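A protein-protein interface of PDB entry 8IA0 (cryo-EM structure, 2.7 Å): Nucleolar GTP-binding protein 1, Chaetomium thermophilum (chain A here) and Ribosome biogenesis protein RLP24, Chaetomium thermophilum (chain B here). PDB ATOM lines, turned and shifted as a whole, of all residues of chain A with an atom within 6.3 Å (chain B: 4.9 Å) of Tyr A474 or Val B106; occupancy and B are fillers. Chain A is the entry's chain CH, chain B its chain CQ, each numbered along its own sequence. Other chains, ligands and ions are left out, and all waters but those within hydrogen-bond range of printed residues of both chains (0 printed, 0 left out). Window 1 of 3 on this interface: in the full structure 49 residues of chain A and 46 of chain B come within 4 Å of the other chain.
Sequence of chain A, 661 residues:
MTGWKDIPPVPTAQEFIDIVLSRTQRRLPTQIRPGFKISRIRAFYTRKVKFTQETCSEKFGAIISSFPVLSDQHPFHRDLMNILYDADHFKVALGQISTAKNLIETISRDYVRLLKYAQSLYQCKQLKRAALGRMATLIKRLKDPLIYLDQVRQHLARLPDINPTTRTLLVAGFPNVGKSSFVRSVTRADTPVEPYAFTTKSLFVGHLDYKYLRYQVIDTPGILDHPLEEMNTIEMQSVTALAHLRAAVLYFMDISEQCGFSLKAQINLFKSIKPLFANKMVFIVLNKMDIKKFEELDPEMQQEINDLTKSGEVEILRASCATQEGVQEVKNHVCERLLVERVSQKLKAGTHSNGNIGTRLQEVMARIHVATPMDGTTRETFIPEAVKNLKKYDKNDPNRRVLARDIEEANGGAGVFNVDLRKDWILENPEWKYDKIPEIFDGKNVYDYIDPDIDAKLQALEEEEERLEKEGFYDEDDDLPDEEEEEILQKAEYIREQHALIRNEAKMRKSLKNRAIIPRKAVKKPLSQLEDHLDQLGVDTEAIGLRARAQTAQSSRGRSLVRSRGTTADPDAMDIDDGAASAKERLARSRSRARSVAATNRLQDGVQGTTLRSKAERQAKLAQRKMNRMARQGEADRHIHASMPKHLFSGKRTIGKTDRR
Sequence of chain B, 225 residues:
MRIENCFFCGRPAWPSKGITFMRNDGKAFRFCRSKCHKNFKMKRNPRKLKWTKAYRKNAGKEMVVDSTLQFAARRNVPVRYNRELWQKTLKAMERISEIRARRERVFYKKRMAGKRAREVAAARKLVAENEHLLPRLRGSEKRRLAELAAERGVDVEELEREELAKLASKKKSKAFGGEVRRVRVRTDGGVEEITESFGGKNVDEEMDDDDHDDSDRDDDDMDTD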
ATOM      1  N   GLU A 464      -7.787 -29.822  12.645  1.00  0.00           N
ATOM      2  CA  GLU A 464      -8.321 -29.620  13.986  1.00  0.00           C
ATOM      3  C   GLU A 464      -8.457 -28.138  14.303  1.00  0.00           C
ATOM      4  O   GLU A 464      -9.401 -27.725  14.987  1.00  0.00           O
ATOM      5  CB  GLU A 464      -7.428 -30.314  15.013  1.00  0.00           C
ATOM      6  CG  GLU A 464      -7.930 -30.226  16.443  1.00  0.00           C
ATOM      7  CD  GLU A 464      -7.036 -30.967  17.418  1.00  0.00           C
ATOM      8  OE1 GLU A 464      -6.005 -31.519  16.981  1.00  0.00           O
ATOM      9  OE2 GLU A 464      -7.364 -30.999  18.623  1.00  0.00           O
ATOM     10  N   GLU A 465      -7.525 -27.320  13.813  1.00  0.00           N
ATOM     11  CA  GLU A 465      -7.601 -25.885  14.063  1.00  0.00           C
ATOM     12  C   GLU A 465      -8.795 -25.261  13.353  1.00  0.00           C
ATOM     13  O   GLU A 465      -9.499 -24.424  13.928  1.00  0.00           O
ATOM     14  CB  GLU A 465      -6.302 -25.208  13.630  1.00  0.00           C
ATOM     15  CG  GLU A 465      -5.217 -25.222  14.693  1.00  0.00           C
ATOM     16  CD  GLU A 465      -5.730 -24.793  16.052  1.00  0.00           C
ATOM     17  OE1 GLU A 465      -5.985 -23.585  16.239  1.00  0.00           O
ATOM     18  OE2 GLU A 465      -5.874 -25.664  16.936  1.00  0.00           O
ATOM     19  N   LEU A 468     -11.915 -26.295  15.170  1.00  0.00           N
ATOM     20  CA  LEU A 468     -12.015 -25.592  16.446  1.00  0.00           C
ATOM     21  C   LEU A 468     -12.340 -24.118  16.235  1.00  0.00           C
ATOM     22  O   LEU A 468     -13.034 -23.499  17.050  1.00  0.00           O
ATOM     23  CB  LEU A 468     -10.719 -25.755  17.238  1.00  0.00           C
ATOM     24  CG  LEU A 468     -10.526 -27.082  17.972  1.00  0.00           C
ATOM     25  CD1 LEU A 468      -9.300 -27.021  18.868  1.00  0.00           C
ATOM     26  CD2 LEU A 468     -11.764 -27.440  18.777  1.00  0.00           C
ATOM     27  N   GLU A 469     -11.831 -23.532  15.151  1.00  0.00           N
ATOM     28  CA  GLU A 469     -12.206 -22.163  14.818  1.00  0.00           C
ATOM     29  C   GLU A 469     -13.638 -22.088  14.310  1.00  0.00           C
ATOM     30  O   GLU A 469     -14.233 -21.005  14.285  1.00  0.00           O
ATOM     31  CB  GLU A 469     -11.244 -21.590  13.777  1.00  0.00           C
ATOM     32  CG  GLU A 469     -10.982 -20.103  13.932  1.00  0.00           C
ATOM     33  CD  GLU A 469      -9.995 -19.573  12.910  1.00  0.00           C
ATOM     34  OE1 GLU A 469      -9.256 -20.386  12.317  1.00  0.00           O
ATOM     35  OE2 GLU A 469      -9.960 -18.341  12.700  1.00  0.00           O
ATOM     36  N   GLU A 471     -16.629 -24.212  15.274  1.00  0.00           N
ATOM     37  CA  GLU A 471     -17.726 -24.350  16.223  1.00  0.00           C
ATOM     38  C   GLU A 471     -17.676 -23.325  17.350  1.00  0.00           C
ATOM     39  O   GLU A 471     -18.685 -23.136  18.037  1.00  0.00           O
ATOM     40  CB  GLU A 471     -17.763 -25.776  16.791  1.00  0.00           C
ATOM     41  CG  GLU A 471     -17.250 -25.966  18.221  1.00  0.00           C
ATOM     42  CD  GLU A 471     -15.766 -25.689  18.393  1.00  0.00           C
ATOM     43  OE1 GLU A 471     -15.103 -25.259  17.428  1.00  0.00           O
ATOM     44  OE2 GLU A 471     -15.261 -25.916  19.512  1.00  0.00           O
ATOM     45  N   GLY A 472     -16.544 -22.655  17.557  1.00  0.00           N
ATOM     46  CA  GLY A 472     -16.517 -21.539  18.482  1.00  0.00           C
ATOM     47  C   GLY A 472     -15.686 -21.762  19.726  1.00  0.00           C
ATOM     48  O   GLY A 472     -16.032 -21.273  20.805  1.00  0.00           O
ATOM     49  N   PHE A 473     -14.598 -22.522  19.600  1.00  0.00           N
ATOM     50  CA  PHE A 473     -13.756 -22.797  20.755  1.00  0.00           C
ATOM     51  C   PHE A 473     -12.840 -21.616  21.061  1.00  0.00           C
ATOM     52  O   PHE A 473     -12.368 -21.491  22.196  1.00  0.00           O
ATOM     53  CB  PHE A 473     -12.976 -24.095  20.503  1.00  0.00           C
ATOM     54  CG  PHE A 473     -11.978 -24.458  21.571  1.00  0.00           C
ATOM     55  CD1 PHE A 473     -10.711 -23.904  21.612  1.00  0.00           C
ATOM     56  CD2 PHE A 473     -12.307 -25.426  22.505  1.00  0.00           C
ATOM     57  CE1 PHE A 473      -9.809 -24.280  22.597  1.00  0.00           C
ATOM     58  CE2 PHE A 473     -11.412 -25.806  23.484  1.00  0.00           C
ATOM     59  CZ  PHE A 473     -10.163 -25.233  23.531  1.00  0.00           C
ATOM     60  N   TYR A 474     -12.634 -20.718  20.087  1.00  0.00           N
ATOM     61  CA  TYR A 474     -11.732 -19.578  20.222  1.00  0.00           C
ATOM     62  C   TYR A 474     -12.467 -18.249  20.074  1.00  0.00           C
ATOM     63  O   TYR A 474     -11.929 -17.297  19.500  1.00  0.00           O
ATOM     64  CB  TYR A 474     -10.603 -19.658  19.198  1.00  0.00           C
ATOM     65  CG  TYR A 474      -9.752 -20.891  19.316  1.00  0.00           C
ATOM     66  CD1 TYR A 474      -8.834 -21.035  20.334  1.00  0.00           C
ATOM     67  CD2 TYR A 474      -9.851 -21.907  18.389  1.00  0.00           C
ATOM     68  CE1 TYR A 474      -8.048 -22.166  20.424  1.00  0.00           C
ATOM     69  CE2 TYR A 474      -9.067 -23.028  18.476  1.00  0.00           C
ATOM     70  CZ  TYR A 474      -8.173 -23.153  19.491  1.00  0.00           C
ATOM     71  OH  TYR A 474      -7.399 -24.280  19.569  1.00  0.00           O
ATOM     72  N   ASP A 475     -13.690 -18.154  20.582  1.00  0.00           N
ATOM     73  CA  ASP A 475     -14.452 -16.915  20.516  1.00  0.00           C
ATOM     74  C   ASP A 475     -14.418 -16.215  21.870  1.00  0.00           C
ATOM     75  O   ASP A 475     -14.575 -16.855  22.916  1.00  0.00           O
ATOM     76  CB  ASP A 475     -15.891 -17.174  20.059  1.00  0.00           C
ATOM     77  CG  ASP A 475     -16.665 -18.065  21.008  1.00  0.00           C
ATOM     78  OD1 ASP A 475     -16.036 -18.766  21.826  1.00  0.00           O
ATOM     79  OD2 ASP A 475     -17.911 -18.072  20.923  1.00  0.00           O
ATOM     80  N   GLU A 476     -14.179 -14.909  21.848  1.00  0.00           N
ATOM     81  CA  GLU A 476     -14.127 -14.113  23.065  1.00  0.00           C
ATOM     82  C   GLU A 476     -15.513 -13.551  23.358  1.00  0.00           C
ATOM     83  O   GLU A 476     -16.109 -12.876  22.510  1.00  0.00           O
ATOM     84  CB  GLU A 476     -13.101 -12.990  22.931  1.00  0.00           C
ATOM     85  CG  GLU A 476     -12.843 -12.242  24.222  1.00  0.00           C
ATOM     86  CD  GLU A 476     -11.741 -11.218  24.083  1.00  0.00           C
ATOM     87  OE1 GLU A 476     -11.171 -11.101  22.976  1.00  0.00           O
ATOM     88  OE2 GLU A 476     -11.445 -10.533  25.083  1.00  0.00           O
ATOM     89  N   ARG B 102      -1.885 -20.348  21.843  1.00  0.00           N
ATOM     90  CA  ARG B 102      -3.230 -19.889  21.522  1.00  0.00           C
ATOM     91  C   ARG B 102      -4.263 -20.977  21.813  1.00  0.00           C
ATOM     92  O   ARG B 102      -5.469 -20.767  21.641  1.00  0.00           O
ATOM     93  CB  ARG B 102      -3.210 -19.366  20.080  1.00  0.00           C
ATOM     94  CG  ARG B 102      -4.473 -18.967  19.322  1.00  0.00           C
ATOM     95  CD  ARG B 102      -4.489 -19.694  17.971  1.00  0.00           C
ATOM     96  NE  ARG B 102      -5.502 -19.209  17.044  1.00  0.00           N
ATOM     97  CZ  ARG B 102      -6.730 -19.685  16.976  1.00  0.00           C
ATOM     98  NH1 ARG B 102      -7.136 -20.641  17.778  1.00  0.00           N
ATOM     99  NH2 ARG B 102      -7.562 -19.204  16.064  1.00  0.00           N
ATOM    100  N   ARG B 103      -3.804 -22.142  22.287  1.00  0.00           N
ATOM    101  CA  ARG B 103      -4.677 -23.061  23.012  1.00  0.00           C
ATOM    102  C   ARG B 103      -4.536 -22.904  24.519  1.00  0.00           C
ATOM    103  O   ARG B 103      -5.507 -23.111  25.252  1.00  0.00           O
ATOM    104  CB  ARG B 103      -4.390 -24.509  22.626  1.00  0.00           C
ATOM    105  CG  ARG B 103      -4.882 -24.906  21.251  1.00  0.00           C
ATOM    106  CD  ARG B 103      -4.626 -26.372  20.978  1.00  0.00           C
ATOM    107  NE  ARG B 103      -5.162 -26.782  19.686  1.00  0.00           N
ATOM    108  CZ  ARG B 103      -4.975 -27.976  19.145  1.00  0.00           C
ATOM    109  NH1 ARG B 103      -4.273 -28.911  19.764  1.00  0.00           N
ATOM    110  NH2 ARG B 103      -5.495 -28.235  17.949  1.00  0.00           N
ATOM    111  N   GLU B 104      -3.341 -22.553  24.999  1.00  0.00           N
ATOM    112  CA  GLU B 104      -3.137 -22.390  26.436  1.00  0.00           C
ATOM    113  C   GLU B 104      -3.881 -21.172  26.967  1.00  0.00           C
ATOM    114  O   GLU B 104      -4.280 -21.144  28.137  1.00  0.00           O
ATOM    115  CB  GLU B 104      -1.641 -22.292  26.748  1.00  0.00           C
ATOM    116  CG  GLU B 104      -1.291 -22.304  28.230  1.00  0.00           C
ATOM    117  CD  GLU B 104      -1.247 -20.912  28.830  1.00  0.00           C
ATOM    118  OE1 GLU B 104      -0.994 -19.944  28.081  1.00  0.00           O
ATOM    119  OE2 GLU B 104      -1.466 -20.787  30.054  1.00  0.00           O
ATOM    120  N   ARG B 105      -4.065 -20.150  26.128  1.00  0.00           N
ATOM    121  CA  ARG B 105      -4.797 -18.961  26.549  1.00  0.00           C
ATOM    122  C   ARG B 105      -6.244 -19.298  26.886  1.00  0.00           C
ATOM    123  O   ARG B 105      -6.812 -18.752  27.839  1.00  0.00           O
ATOM    124  CB  ARG B 105      -4.732 -17.897  25.454  1.00  0.00           C
ATOM    125  CG  ARG B 105      -5.492 -16.625  25.768  1.00  0.00           C
ATOM    126  CD  ARG B 105      -4.983 -15.977  27.048  1.00  0.00           C
ATOM    127  NE  ARG B 105      -3.973 -14.950  26.805  1.00  0.00           N
ATOM    128  CZ  ARG B 105      -4.184 -13.815  26.151  1.00  0.00           C
ATOM    129  NH1 ARG B 105      -5.380 -13.496  25.680  1.00  0.00           N
ATOM    130  NH2 ARG B 105      -3.172 -12.971  25.974  1.00  0.00           N
ATOM    131  N   VAL B 106      -6.858 -20.192  26.111  1.00  0.00           N
ATOM    132  CA  VAL B 106      -8.221 -20.623  26.402  1.00  0.00           C
ATOM    133  C   VAL B 106      -8.263 -21.408  27.706  1.00  0.00           C
ATOM    134  O   VAL B 106      -9.218 -21.301  28.485  1.00  0.00           O
ATOM    135  CB  VAL B 106      -8.778 -21.438  25.220  1.00  0.00           C
ATOM    136  CG1 VAL B 106      -9.817 -22.442  25.689  1.00  0.00           C
ATOM    137  CG2 VAL B 106      -9.367 -20.511  24.171  1.00  0.00           C
ATOM    138  N   PHE B 107      -7.219 -22.195  27.976  1.00  0.00           N
ATOM    139  CA  PHE B 107      -7.176 -22.993  29.196  1.00  0.00           C
ATOM    140  C   PHE B 107      -7.209 -22.109  30.436  1.00  0.00           C
ATOM    141  O   PHE B 107      -7.915 -22.406  31.406  1.00  0.00           O
ATOM    142  CB  PHE B 107      -5.927 -23.873  29.199  1.00  0.00           C
ATOM    143  CG  PHE B 107      -5.969 -24.982  30.206  1.00  0.00           C
ATOM    144  CD1 PHE B 107      -6.655 -26.153  29.942  1.00  0.00           C
ATOM    145  CD2 PHE B 107      -5.316 -24.855  31.418  1.00  0.00           C
ATOM    146  CE1 PHE B 107      -6.692 -27.174  30.869  1.00  0.00           C
ATOM    147  CE2 PHE B 107      -5.349 -25.872  32.347  1.00  0.00           C
ATOM    148  CZ  PHE B 107      -6.037 -27.034  32.072  1.00  0.00           C
ATOM    149  N   TYR B 108      -6.442 -21.020  30.426  1.00  0.00           N
ATOM    150  CA  TYR B 108      -6.425 -20.120  31.573  1.00  0.00           C
ATOM    151  C   TYR B 108      -7.765 -19.420  31.748  1.00  0.00           C
ATOM    152  O   TYR B 108      -8.264 -19.294  32.872  1.00  0.00           O
ATOM    153  CB  TYR B 108      -5.307 -19.096  31.413  1.00  0.00           C
ATOM    154  CG  TYR B 108      -4.925 -18.390  32.690  1.00  0.00           C
ATOM    155  CD1 TYR B 108      -4.394 -19.092  33.760  1.00  0.00           C
ATOM    156  CD2 TYR B 108      -5.088 -17.020  32.823  1.00  0.00           C
ATOM    157  CE1 TYR B 108      -4.040 -18.451  34.928  1.00  0.00           C
ATOM    158  CE2 TYR B 108      -4.738 -16.370  33.986  1.00  0.00           C
ATOM    159  CZ  TYR B 108      -4.215 -17.090  35.035  1.00  0.00           C
ATOM    160  OH  TYR B 108      -3.861 -16.445  36.198  1.00  0.00           O
ATOM    161  N   LYS B 109      -8.365 -18.962  30.649  1.00  0.00           N
ATOM    162  CA  LYS B 109      -9.649 -18.278  30.740  1.00  0.00           C
ATOM    163  C   LYS B 109     -10.734 -19.212  31.261  1.00  0.00           C
ATOM    164  O   LYS B 109     -11.629 -18.783  31.999  1.00  0.00           O
ATOM    165  CB  LYS B 109     -10.036 -17.707  29.378  1.00  0.00           C
ATOM    166  CG  LYS B 109      -9.456 -16.334  29.098  1.00  0.00           C
ATOM    167  CD  LYS B 109     -10.207 -15.641  27.977  1.00  0.00           C
ATOM    168  CE  LYS B 109     -10.103 -14.132  28.093  1.00  0.00           C
ATOM    169  NZ  LYS B 109     -10.603 -13.642  29.406  1.00  0.00           N
ATOM    170  N   LYS B 110     -10.674 -20.490  30.886  1.00  0.00           N
ATOM    171  CA  LYS B 110     -11.641 -21.455  31.395  1.00  0.00           C
ATOM    172  C   LYS B 110     -11.459 -21.683  32.892  1.00  0.00           C
ATOM    173  O   LYS B 110     -12.441 -21.850  33.624  1.00  0.00           O
ATOM    174  CB  LYS B 110     -11.517 -22.771  30.631  1.00  0.00           C
ATOM    175  CG  LYS B 110     -12.342 -22.824  29.355  1.00  0.00           C
ATOM    176  CD  LYS B 110     -12.676 -24.256  28.960  1.00  0.00           C
ATOM    177  CE  LYS B 110     -13.536 -24.962  30.004  1.00  0.00           C
ATOM    178  NZ  LYS B 110     -14.386 -24.034  30.807  1.00  0.00           N
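OE2 of Glu A464 is in salt-bridge range of NH2 of Arg B103, 3.4 Å away. The side-chain carboxylate (OE1) of Glu A465 lies within salt-bridge range of the guanidinium group (NH1) of Arg B102. The guanidinium group (NH2) of Arg B103 lies within salt-bridge range of the side-chain carboxylate (OE2) of Glu A465. The side-chain hydroxyl (OH) of Tyr A474 sits close to the guanidinium group (NE) of Arg B103.
The side-chain carboxylate (OE2) of Glu A465 sits at hydrogen-bond distance from the side-chain hydroxyl (OH) of Tyr A474 (3.3 Å). The backbone NH (N) of Phe A473 lies within hydrogen-bond range of the backbone carbonyl oxygen (O) of Leu A468, 3.1 Å away. The side-chain carboxylate (OE2) of Glu A471 lies close to the backbone NH (N) of Phe A473, at 3.5 Å.
Among the printed residues, pairs that only touch across the chains: Phe A473 with Val B106, Tyr A474 with Arg B102 and Tyr A474 with Val B106.
Tyr A474 touches just these residues of chain B: Arg B102, Arg B103 and Val B106. Of the printed residues of chain B, Glu A464 touches Arg B103 (3.2 Å). Printed residues of chain B within 4 Å of Phe A473: Val B106. Printed residues of chain A within 4 Å of Arg B102: Glu A465 (3.5 Å) and Tyr A474 (3.0 Å). The nearest printed residue of chain B that does not touch Tyr A474 is Glu B104 (6.6 Å). The nearest residue of chain A that does not touch Val B106 is Asp A475 (6.1 Å).
Of the 9 printed residues of chain B, 3 touch a printed residue of chain A. Hydrophobic or aromatic side chains of chain B within 4 Å of the printed part of chain A: Val B106. Of the 10 printed residues of chain A, 4 touch a printed residue of chain B. Printed residues of chain A that touch a printed residue of chain B: Glu A464, Glu A465, Phe A473 and Tyr A474.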
